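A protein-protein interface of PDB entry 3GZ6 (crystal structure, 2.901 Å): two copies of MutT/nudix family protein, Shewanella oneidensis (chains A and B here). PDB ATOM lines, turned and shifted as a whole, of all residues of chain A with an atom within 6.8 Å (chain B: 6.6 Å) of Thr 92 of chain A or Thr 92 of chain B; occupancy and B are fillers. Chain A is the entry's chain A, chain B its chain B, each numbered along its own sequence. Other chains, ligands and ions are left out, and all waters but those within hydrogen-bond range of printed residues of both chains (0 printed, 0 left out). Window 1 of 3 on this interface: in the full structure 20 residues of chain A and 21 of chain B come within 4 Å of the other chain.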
ATOM      1  N   LEU A  23      -9.387  -9.793  26.331  1.00  0.00           N
ATOM      2  CA  LEU A  23     -10.589  -9.510  27.083  1.00  0.00           C
ATOM      3  C   LEU A  23     -10.768 -10.532  28.203  1.00  0.00           C
ATOM      4  O   LEU A  23     -10.077 -11.546  28.256  1.00  0.00           O
ATOM      5  CB  LEU A  23     -11.752  -9.591  26.100  1.00  0.00           C
ATOM      6  CG  LEU A  23     -13.194  -9.448  26.541  1.00  0.00           C
ATOM      7  CD1 LEU A  23     -13.428  -8.048  27.030  1.00  0.00           C
ATOM      8  CD2 LEU A  23     -14.071  -9.748  25.358  1.00  0.00           C
ATOM      9  N   LEU A  68     -19.978 -15.313  23.899  1.00  0.00           N
ATOM     10  CA  LEU A  68     -19.468 -14.836  25.185  1.00  0.00           C
ATOM     11  C   LEU A  68     -20.077 -15.634  26.323  1.00  0.00           C
ATOM     12  O   LEU A  68     -19.385 -16.030  27.258  1.00  0.00           O
ATOM     13  CB  LEU A  68     -19.760 -13.338  25.381  1.00  0.00           C
ATOM     14  CG  LEU A  68     -18.810 -12.371  24.659  1.00  0.00           C
ATOM     15  CD1 LEU A  68     -19.211 -10.924  24.837  1.00  0.00           C
ATOM     16  CD2 LEU A  68     -17.386 -12.568  25.138  1.00  0.00           C
ATOM     17  N   GLN A  89     -26.354 -10.937  31.346  1.00  0.00           N
ATOM     18  CA  GLN A  89     -25.149 -10.121  31.212  1.00  0.00           C
ATOM     19  C   GLN A  89     -25.369  -8.838  31.995  1.00  0.00           C
ATOM     20  O   GLN A  89     -26.429  -8.233  31.887  1.00  0.00           O
ATOM     21  CB  GLN A  89     -24.947  -9.796  29.738  1.00  0.00           C
ATOM     22  CG  GLN A  89     -23.559  -9.451  29.312  1.00  0.00           C
ATOM     23  CD  GLN A  89     -23.554  -8.962  27.889  1.00  0.00           C
ATOM     24  OE1 GLN A  89     -23.187  -9.690  26.975  1.00  0.00           O
ATOM     25  NE2 GLN A  89     -24.000  -7.727  27.688  1.00  0.00           N
ATOM     26  N   LEU A  90     -24.393  -8.428  32.799  1.00  0.00           N
ATOM     27  CA  LEU A  90     -24.596  -7.314  33.716  1.00  0.00           C
ATOM     28  C   LEU A  90     -24.162  -6.029  33.069  1.00  0.00           C
ATOM     29  O   LEU A  90     -24.911  -5.062  32.990  1.00  0.00           O
ATOM     30  CB  LEU A  90     -23.788  -7.525  34.992  1.00  0.00           C
ATOM     31  CG  LEU A  90     -23.863  -6.393  36.024  1.00  0.00           C
ATOM     32  CD1 LEU A  90     -25.291  -6.215  36.481  1.00  0.00           C
ATOM     33  CD2 LEU A  90     -22.965  -6.667  37.212  1.00  0.00           C
ATOM     34  N   CYS A  91     -22.927  -6.024  32.609  1.00  0.00           N
ATOM     35  CA  CYS A  91     -22.381  -4.854  31.965  1.00  0.00           C
ATOM     36  C   CYS A  91     -20.963  -5.189  31.604  1.00  0.00           C
ATOM     37  O   CYS A  91     -20.454  -6.232  31.993  1.00  0.00           O
ATOM     38  CB  CYS A  91     -22.370  -3.689  32.937  1.00  0.00           C
ATOM     39  SG  CYS A  91     -21.194  -3.934  34.263  1.00  0.00           S
ATOM     40  N   THR A  92     -20.328  -4.294  30.865  1.00  0.00           N
ATOM     41  CA  THR A  92     -18.947  -4.469  30.477  1.00  0.00           C
ATOM     42  C   THR A  92     -18.143  -3.289  30.955  1.00  0.00           C
ATOM     43  O   THR A  92     -18.481  -2.155  30.662  1.00  0.00           O
ATOM     44  CB  THR A  92     -18.827  -4.544  28.968  1.00  0.00           C
ATOM     45  OG1 THR A  92     -19.445  -5.754  28.518  1.00  0.00           O
ATOM     46  CG2 THR A  92     -17.366  -4.529  28.556  1.00  0.00           C
ATOM     47  N   VAL A  93     -17.080  -3.551  31.697  1.00  0.00           N
ATOM     48  CA  VAL A  93     -16.251  -2.470  32.201  1.00  0.00           C
ATOM     49  C   VAL A  93     -14.939  -2.435  31.442  1.00  0.00           C
ATOM     50  O   VAL A  93     -14.318  -3.469  31.205  1.00  0.00           O
ATOM     51  CB  VAL A  93     -15.972  -2.616  33.702  1.00  0.00           C
ATOM     52  CG1 VAL A  93     -15.142  -1.457  34.188  1.00  0.00           C
ATOM     53  CG2 VAL A  93     -17.269  -2.670  34.466  1.00  0.00           C
ATOM     54  N   GLY A  94     -14.513  -1.241  31.060  1.00  0.00           N
ATOM     55  CA  GLY A  94     -13.267  -1.106  30.340  1.00  0.00           C
ATOM     56  C   GLY A  94     -12.683   0.276  30.482  1.00  0.00           C
ATOM     57  O   GLY A  94     -13.330   1.279  30.170  1.00  0.00           O
ATOM     58  N   VAL A 105     -10.391  -4.931  29.777  1.00  0.00           N
ATOM     59  CA  VAL A 105     -11.835  -5.054  29.555  1.00  0.00           C
ATOM     60  C   VAL A 105     -12.427  -6.367  30.058  1.00  0.00           C
ATOM     61  O   VAL A 105     -11.976  -7.449  29.680  1.00  0.00           O
ATOM     62  CB  VAL A 105     -12.185  -4.946  28.088  1.00  0.00           C
ATOM     63  CG1 VAL A 105     -13.683  -4.865  27.937  1.00  0.00           C
ATOM     64  CG2 VAL A 105     -11.519  -3.742  27.488  1.00  0.00           C
ATOM     65  N   THR A 106     -13.440  -6.261  30.909  1.00  0.00           N
ATOM     66  CA  THR A 106     -14.157  -7.432  31.399  1.00  0.00           C
ATOM     67  C   THR A 106     -15.622  -7.334  31.023  1.00  0.00           C
ATOM     68  O   THR A 106     -16.259  -6.299  31.203  1.00  0.00           O
ATOM     69  CB  THR A 106     -14.052  -7.592  32.937  1.00  0.00           C
ATOM     70  OG1 THR A 106     -12.759  -8.108  33.278  1.00  0.00           O
ATOM     71  CG2 THR A 106     -15.113  -8.544  33.451  1.00  0.00           C
ATOM     72  N   VAL A 107     -16.143  -8.410  30.462  1.00  0.00           N
ATOM     73  CA  VAL A 107     -17.572  -8.539  30.309  1.00  0.00           C
ATOM     74  C   VAL A 107     -18.075  -9.374  31.468  1.00  0.00           C
ATOM     75  O   VAL A 107     -17.692 -10.530  31.622  1.00  0.00           O
ATOM     76  CB  VAL A 107     -17.940  -9.195  28.977  1.00  0.00           C
ATOM     77  CG1 VAL A 107     -19.459  -9.368  28.866  1.00  0.00           C
ATOM     78  CG2 VAL A 107     -17.387  -8.357  27.824  1.00  0.00           C
ATOM     79  N   CYS A 108     -18.934  -8.774  32.280  1.00  0.00           N
ATOM     80  CA  CYS A 108     -19.395  -9.388  33.512  1.00  0.00           C
ATOM     81  C   CYS A 108     -20.870  -9.770  33.463  1.00  0.00           C
ATOM     82  O   CYS A 108     -21.704  -8.988  33.006  1.00  0.00           O
ATOM     83  CB  CYS A 108     -19.143  -8.437  34.683  1.00  0.00           C
ATOM     84  SG  CYS A 108     -19.691  -9.046  36.269  1.00  0.00           S
ATOM     85  N   TYR A 109     -21.168 -10.978  33.951  1.00  0.00           N
ATOM     86  CA  TYR A 109     -22.529 -11.512  34.056  1.00  0.00           C
ATOM     87  C   TYR A 109     -23.008 -11.617  35.505  1.00  0.00           C
ATOM     88  O   TYR A 109     -22.219 -11.515  36.444  1.00  0.00           O
ATOM     89  CB  TYR A 109     -22.581 -12.906  33.438  1.00  0.00           C
ATOM     90  CG  TYR A 109     -22.434 -12.929  31.946  1.00  0.00           C
ATOM     91  CD1 TYR A 109     -23.519 -13.218  31.131  1.00  0.00           C
ATOM     92  CD2 TYR A 109     -21.218 -12.654  31.344  1.00  0.00           C
ATOM     93  CE1 TYR A 109     -23.394 -13.239  29.755  1.00  0.00           C
ATOM     94  CE2 TYR A 109     -21.084 -12.665  29.963  1.00  0.00           C
ATOM     95  CZ  TYR A 109     -22.177 -12.959  29.174  1.00  0.00           C
ATOM     96  OH  TYR A 109     -22.059 -12.978  27.801  1.00  0.00           O
ATOM     97  N   LEU A 148     -18.354  -4.415  40.849  1.00  0.00           N
ATOM     98  CA  LEU A 148     -19.134  -5.345  40.044  1.00  0.00           C
ATOM     99  C   LEU A 148     -20.147  -6.085  40.909  1.00  0.00           C
ATOM    100  O   LEU A 148     -21.342  -6.124  40.606  1.00  0.00           O
ATOM    101  CB  LEU A 148     -18.219  -6.329  39.314  1.00  0.00           C
ATOM    102  CG  LEU A 148     -17.376  -5.732  38.174  1.00  0.00           C
ATOM    103  CD1 LEU A 148     -16.409  -6.737  37.624  1.00  0.00           C
ATOM    104  CD2 LEU A 148     -18.235  -5.206  37.047  1.00  0.00           C
ATOM    105  N   LEU B  23     -11.298  -5.113  19.669  1.00  0.00           N
ATOM    106  CA  LEU B  23     -12.666  -4.957  20.101  1.00  0.00           C
ATOM    107  C   LEU B  23     -13.275  -3.719  19.453  1.00  0.00           C
ATOM    108  O   LEU B  23     -12.561  -2.818  19.007  1.00  0.00           O
ATOM    109  CB  LEU B  23     -12.650  -4.800  21.620  1.00  0.00           C
ATOM    110  CG  LEU B  23     -13.915  -4.368  22.337  1.00  0.00           C
ATOM    111  CD1 LEU B  23     -14.898  -5.503  22.296  1.00  0.00           C
ATOM    112  CD2 LEU B  23     -13.576  -4.023  23.753  1.00  0.00           C
ATOM    113  N   LEU B  68     -14.495   2.951  28.129  1.00  0.00           N
ATOM    114  CA  LEU B  68     -15.289   2.537  26.969  1.00  0.00           C
ATOM    115  C   LEU B  68     -16.255   3.639  26.563  1.00  0.00           C
ATOM    116  O   LEU B  68     -16.439   3.905  25.381  1.00  0.00           O
ATOM    117  CB  LEU B  68     -16.070   1.244  27.259  1.00  0.00           C
ATOM    118  CG  LEU B  68     -15.264  -0.062  27.306  1.00  0.00           C
ATOM    119  CD1 LEU B  68     -16.102  -1.237  27.747  1.00  0.00           C
ATOM    120  CD2 LEU B  68     -14.653  -0.366  25.965  1.00  0.00           C
ATOM    121  N   GLN B  89     -25.229   1.936  28.265  1.00  0.00           N
ATOM    122  CA  GLN B  89     -24.629   0.745  27.670  1.00  0.00           C
ATOM    123  C   GLN B  89     -25.736  -0.250  27.423  1.00  0.00           C
ATOM    124  O   GLN B  89     -26.576  -0.459  28.291  1.00  0.00           O
ATOM    125  CB  GLN B  89     -23.606   0.140  28.613  1.00  0.00           C
ATOM    126  CG  GLN B  89     -22.553  -0.699  27.941  1.00  0.00           C
ATOM    127  CD  GLN B  89     -21.538  -1.211  28.932  1.00  0.00           C
ATOM    128  OE1 GLN B  89     -20.356  -0.908  28.835  1.00  0.00           O
ATOM    129  NE2 GLN B  89     -22.001  -1.977  29.910  1.00  0.00           N
ATOM    130  N   LEU B  90     -25.762  -0.849  26.236  1.00  0.00           N
ATOM    131  CA  LEU B  90     -26.888  -1.698  25.857  1.00  0.00           C
ATOM    132  C   LEU B  90     -26.578  -3.150  26.122  1.00  0.00           C
ATOM    133  O   LEU B  90     -27.296  -3.844  26.836  1.00  0.00           O
ATOM    134  CB  LEU B  90     -27.225  -1.528  24.376  1.00  0.00           C
ATOM    135  CG  LEU B  90     -28.408  -2.407  23.946  1.00  0.00           C
ATOM    136  CD1 LEU B  90     -29.673  -1.924  24.626  1.00  0.00           C
ATOM    137  CD2 LEU B  90     -28.591  -2.429  22.440  1.00  0.00           C
ATOM    138  N   CYS B  91     -25.501  -3.609  25.512  1.00  0.00           N
ATOM    139  CA  CYS B  91     -25.052  -4.958  25.734  1.00  0.00           C
ATOM    140  C   CYS B  91     -23.766  -5.132  24.983  1.00  0.00           C
ATOM    141  O   CYS B  91     -23.344  -4.232  24.266  1.00  0.00           O
ATOM    142  CB  CYS B  91     -26.081  -5.940  25.202  1.00  0.00           C
ATOM    143  SG  CYS B  91     -26.189  -5.930  23.430  1.00  0.00           S
ATOM    144  N   THR B  92     -23.146  -6.289  25.158  1.00  0.00           N
ATOM    145  CA  THR B  92     -21.952  -6.633  24.413  1.00  0.00           C
ATOM    146  C   THR B  92     -22.184  -7.924  23.666  1.00  0.00           C
ATOM    147  O   THR B  92     -22.635  -8.897  24.242  1.00  0.00           O
ATOM    148  CB  THR B  92     -20.760  -6.812  25.344  1.00  0.00           C
ATOM    149  OG1 THR B  92     -20.464  -5.559  25.963  1.00  0.00           O
ATOM    150  CG2 THR B  92     -19.549  -7.276  24.568  1.00  0.00           C
ATOM    151  N   VAL B  93     -21.891  -7.930  22.377  1.00  0.00           N
ATOM    152  CA  VAL B  93     -22.086  -9.134  21.592  1.00  0.00           C
ATOM    153  C   VAL B  93     -20.740  -9.722  21.211  1.00  0.00           C
ATOM    154  O   VAL B  93     -19.827  -9.009  20.797  1.00  0.00           O
ATOM    155  CB  VAL B  93     -22.904  -8.857  20.332  1.00  0.00           C
ATOM    156  CG1 VAL B  93     -23.215 -10.156  19.626  1.00  0.00           C
ATOM    157  CG2 VAL B  93     -24.186  -8.160  20.698  1.00  0.00           C
ATOM    158  N   GLY B  94     -20.612 -11.033  21.343  1.00  0.00           N
ATOM    159  CA  GLY B  94     -19.365 -11.679  21.002  1.00  0.00           C
ATOM    160  C   GLY B  94     -19.556 -13.136  20.671  1.00  0.00           C
ATOM    161  O   GLY B  94     -20.052 -13.916  21.482  1.00  0.00           O
ATOM    162  N   VAL B 105     -15.913  -8.932  18.825  1.00  0.00           N
ATOM    163  CA  VAL B 105     -16.686  -8.418  19.946  1.00  0.00           C
ATOM    164  C   VAL B 105     -17.024  -6.944  19.791  1.00  0.00           C
ATOM    165  O   VAL B 105     -16.186  -6.140  19.374  1.00  0.00           O
ATOM    166  CB  VAL B 105     -15.945  -8.591  21.248  1.00  0.00           C
ATOM    167  CG1 VAL B 105     -16.838  -8.167  22.371  1.00  0.00           C
ATOM    168  CG2 VAL B 105     -15.509 -10.028  21.410  1.00  0.00           C
ATOM    169  N   THR B 106     -18.263  -6.603  20.118  1.00  0.00           N
ATOM    170  CA  THR B 106     -18.708  -5.220  20.087  1.00  0.00           C
ATOM    171  C   THR B 106     -19.395  -4.852  21.391  1.00  0.00           C
ATOM    172  O   THR B 106     -20.278  -5.558  21.867  1.00  0.00           O
ATOM    173  CB  THR B 106     -19.658  -4.933  18.908  1.00  0.00           C
ATOM    174  OG1 THR B 106     -18.892  -4.766  17.707  1.00  0.00           O
ATOM    175  CG2 THR B 106     -20.445  -3.672  19.169  1.00  0.00           C
ATOM    176  N   VAL B 107     -18.947  -3.759  21.990  1.00  0.00           N
ATOM    177  CA  VAL B 107     -19.663  -3.194  23.109  1.00  0.00           C
ATOM    178  C   VAL B 107     -20.572  -2.118  22.559  1.00  0.00           C
ATOM    179  O   VAL B 107     -20.112  -1.089  22.075  1.00  0.00           O
ATOM    180  CB  VAL B 107     -18.722  -2.624  24.176  1.00  0.00           C
ATOM    181  CG1 VAL B 107     -19.526  -2.017  25.322  1.00  0.00           C
ATOM    182  CG2 VAL B 107     -17.809  -3.724  24.697  1.00  0.00           C
ATOM    183  N   CYS B 108     -21.870  -2.375  22.644  1.00  0.00           N
ATOM    184  CA  CYS B 108     -22.877  -1.505  22.073  1.00  0.00           C
ATOM    185  C   CYS B 108     -23.598  -0.634  23.103  1.00  0.00           C
ATOM    186  O   CYS B 108     -23.993  -1.112  24.165  1.00  0.00           O
ATOM    187  CB  CYS B 108     -23.895  -2.355  21.324  1.00  0.00           C
ATOM    188  SG  CYS B 108     -24.996  -1.421  20.285  1.00  0.00           S
ATOM    189  N   TYR B 109     -23.785   0.639  22.751  1.00  0.00           N
ATOM    190  CA  TYR B 109     -24.496   1.614  23.578  1.00  0.00           C
ATOM    191  C   TYR B 109     -25.811   2.069  22.936  1.00  0.00           C
ATOM    192  O   TYR B 109     -26.037   1.853  21.746  1.00  0.00           O
ATOM    193  CB  TYR B 109     -23.606   2.836  23.802  1.00  0.00           C
ATOM    194  CG  TYR B 109     -22.451   2.599  24.735  1.00  0.00           C
ATOM    195  CD1 TYR B 109     -22.503   3.035  26.053  1.00  0.00           C
ATOM    196  CD2 TYR B 109     -21.313   1.922  24.312  1.00  0.00           C
ATOM    197  CE1 TYR B 109     -21.447   2.818  26.921  1.00  0.00           C
ATOM    198  CE2 TYR B 109     -20.248   1.691  25.182  1.00  0.00           C
ATOM    199  CZ  TYR B 109     -20.323   2.147  26.487  1.00  0.00           C
ATOM    200  OH  TYR B 109     -19.279   1.940  27.368  1.00  0.00           O
ATOM    201  N   LEU B 148     -29.012  -5.459  16.835  1.00  0.00           N
ATOM    202  CA  LEU B 148     -28.649  -4.481  17.850  1.00  0.00           C
ATOM    203  C   LEU B 148     -29.653  -3.325  17.876  1.00  0.00           C
ATOM    204  O   LEU B 148     -30.153  -2.940  18.929  1.00  0.00           O
ATOM    205  CB  LEU B 148     -27.220  -3.967  17.619  1.00  0.00           C
ATOM    206  CG  LEU B 148     -26.074  -4.964  17.860  1.00  0.00           C
ATOM    207  CD1 LEU B 148     -24.771  -4.475  17.293  1.00  0.00           C
ATOM    208  CD2 LEU B 148     -25.887  -5.274  19.328  1.00  0.00           C
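The backbone NH (N) of Leu 68 of chain B lies within hydrogen-bond range of the backbone carbonyl oxygen (O) of Gly 94 of chain A. OG1 of Thr 92 of chain A is in hydrogen-bond range of OG1 of Thr 92 of chain B, 2.8 Å away. The backbone carbonyl oxygen of Gly 94 of chain B lies within hydrogen-bond range of the backbone NH of Leu 68 of chain A (2.8 Å). The backbone carbonyl oxygen (O) of Thr 92 of chain A lies close to the side-chain amide oxygen (OE1) of Gln 89 of chain B (2.9 Å). OE1 of Gln 89 of chain A lies close to O of Thr 92 of chain B.
O of Cys 91 of chain B lies within hydrogen-bond range of N of Cys 108 of chain B (2.9 Å). The side-chain amide oxygen (OE1) of Gln 89 of chain B sits at hydrogen-bond distance from the side-chain hydroxyl (OH) of Tyr 109 of chain B, at 3.4 Å. The backbone carbonyl oxygen (O) of Cys 91 of chain A lies within hydrogen-bond range of the backbone NH (N) of Cys 108 of chain A (3.0 Å).
Among the printed residues, merely in contact across the chains: Leu 68 of chain A with Thr 92 of chain B (3.7 Å), Gln 89 of chain A with Cys 91 of chain B (3.5 Å), Cys 91 of chain A with Gln 89 of chain B (3.5 Å), Thr 92 of chain A with Leu 68 of chain B (3.6 Å) and Thr 92 of chain A with Val 107 of chain B (3.97 Å).
Printed residues of chain B within 4 Å of Leu 68 of chain A: Thr 92 (3.7 Å) and Gly 94 (2.8 Å). Of chain B, only Leu 68 (3.6 Å), Gln 89 (2.9 Å), Thr 92 (2.8 Å) and Val 107 (3.97 Å) come within 4 Å of Thr 92 of chain A. Of the printed residues of chain B, Gly 94 of chain A touches Leu 68 (2.9 Å). Of the printed residues of chain A, Gln 89 of chain B touches Cys 91 (3.5 Å) and Thr 92 (2.9 Å). Of the printed residues of chain A, Cys 91 of chain B touches Gln 89. Thr 92 of chain B touches three residues of chain A. The nearest printed residue of chain A that does not touch Val 107 of chain B is Val 105 of chain A (5.4 Å).
Printed residues of chain B that touch a printed residue of chain A: Leu 68, Gln 89, Cys 91, Thr 92, Gly 94 and Val 107. Hydrophobic or aromatic side chains of chain B within 4 Å of the printed part of chain A: Leu 68 and Val 107. Of the 14 printed residues of chain A, 5 touch a printed residue of chain B. Hydrophobic or aromatic side chains of chain A within 4 Å of the printed part of chain B: Leu 68.
Leu 68 of chain A touches Gly 94 of chain B, and with the chains exchanged Gly 94 of chain A touches Leu 68 of chain B. Gln 89 of chain A touches Cys 91 of chain B, and with the chains exchanged Cys 91 of chain A touches Gln 89 of chain B. Gln 89 of chain A touches Thr 92 of chain B, and with the chains exchanged Thr 92 of chain A touches Gln 89 of chain B. Thr 92 of chain A touches Val 107 of chain B, but with the chains exchanged Val 107 of chain A does not touch Thr 92 of chain B (4.1 Å). 14 positions are printed for both chains.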
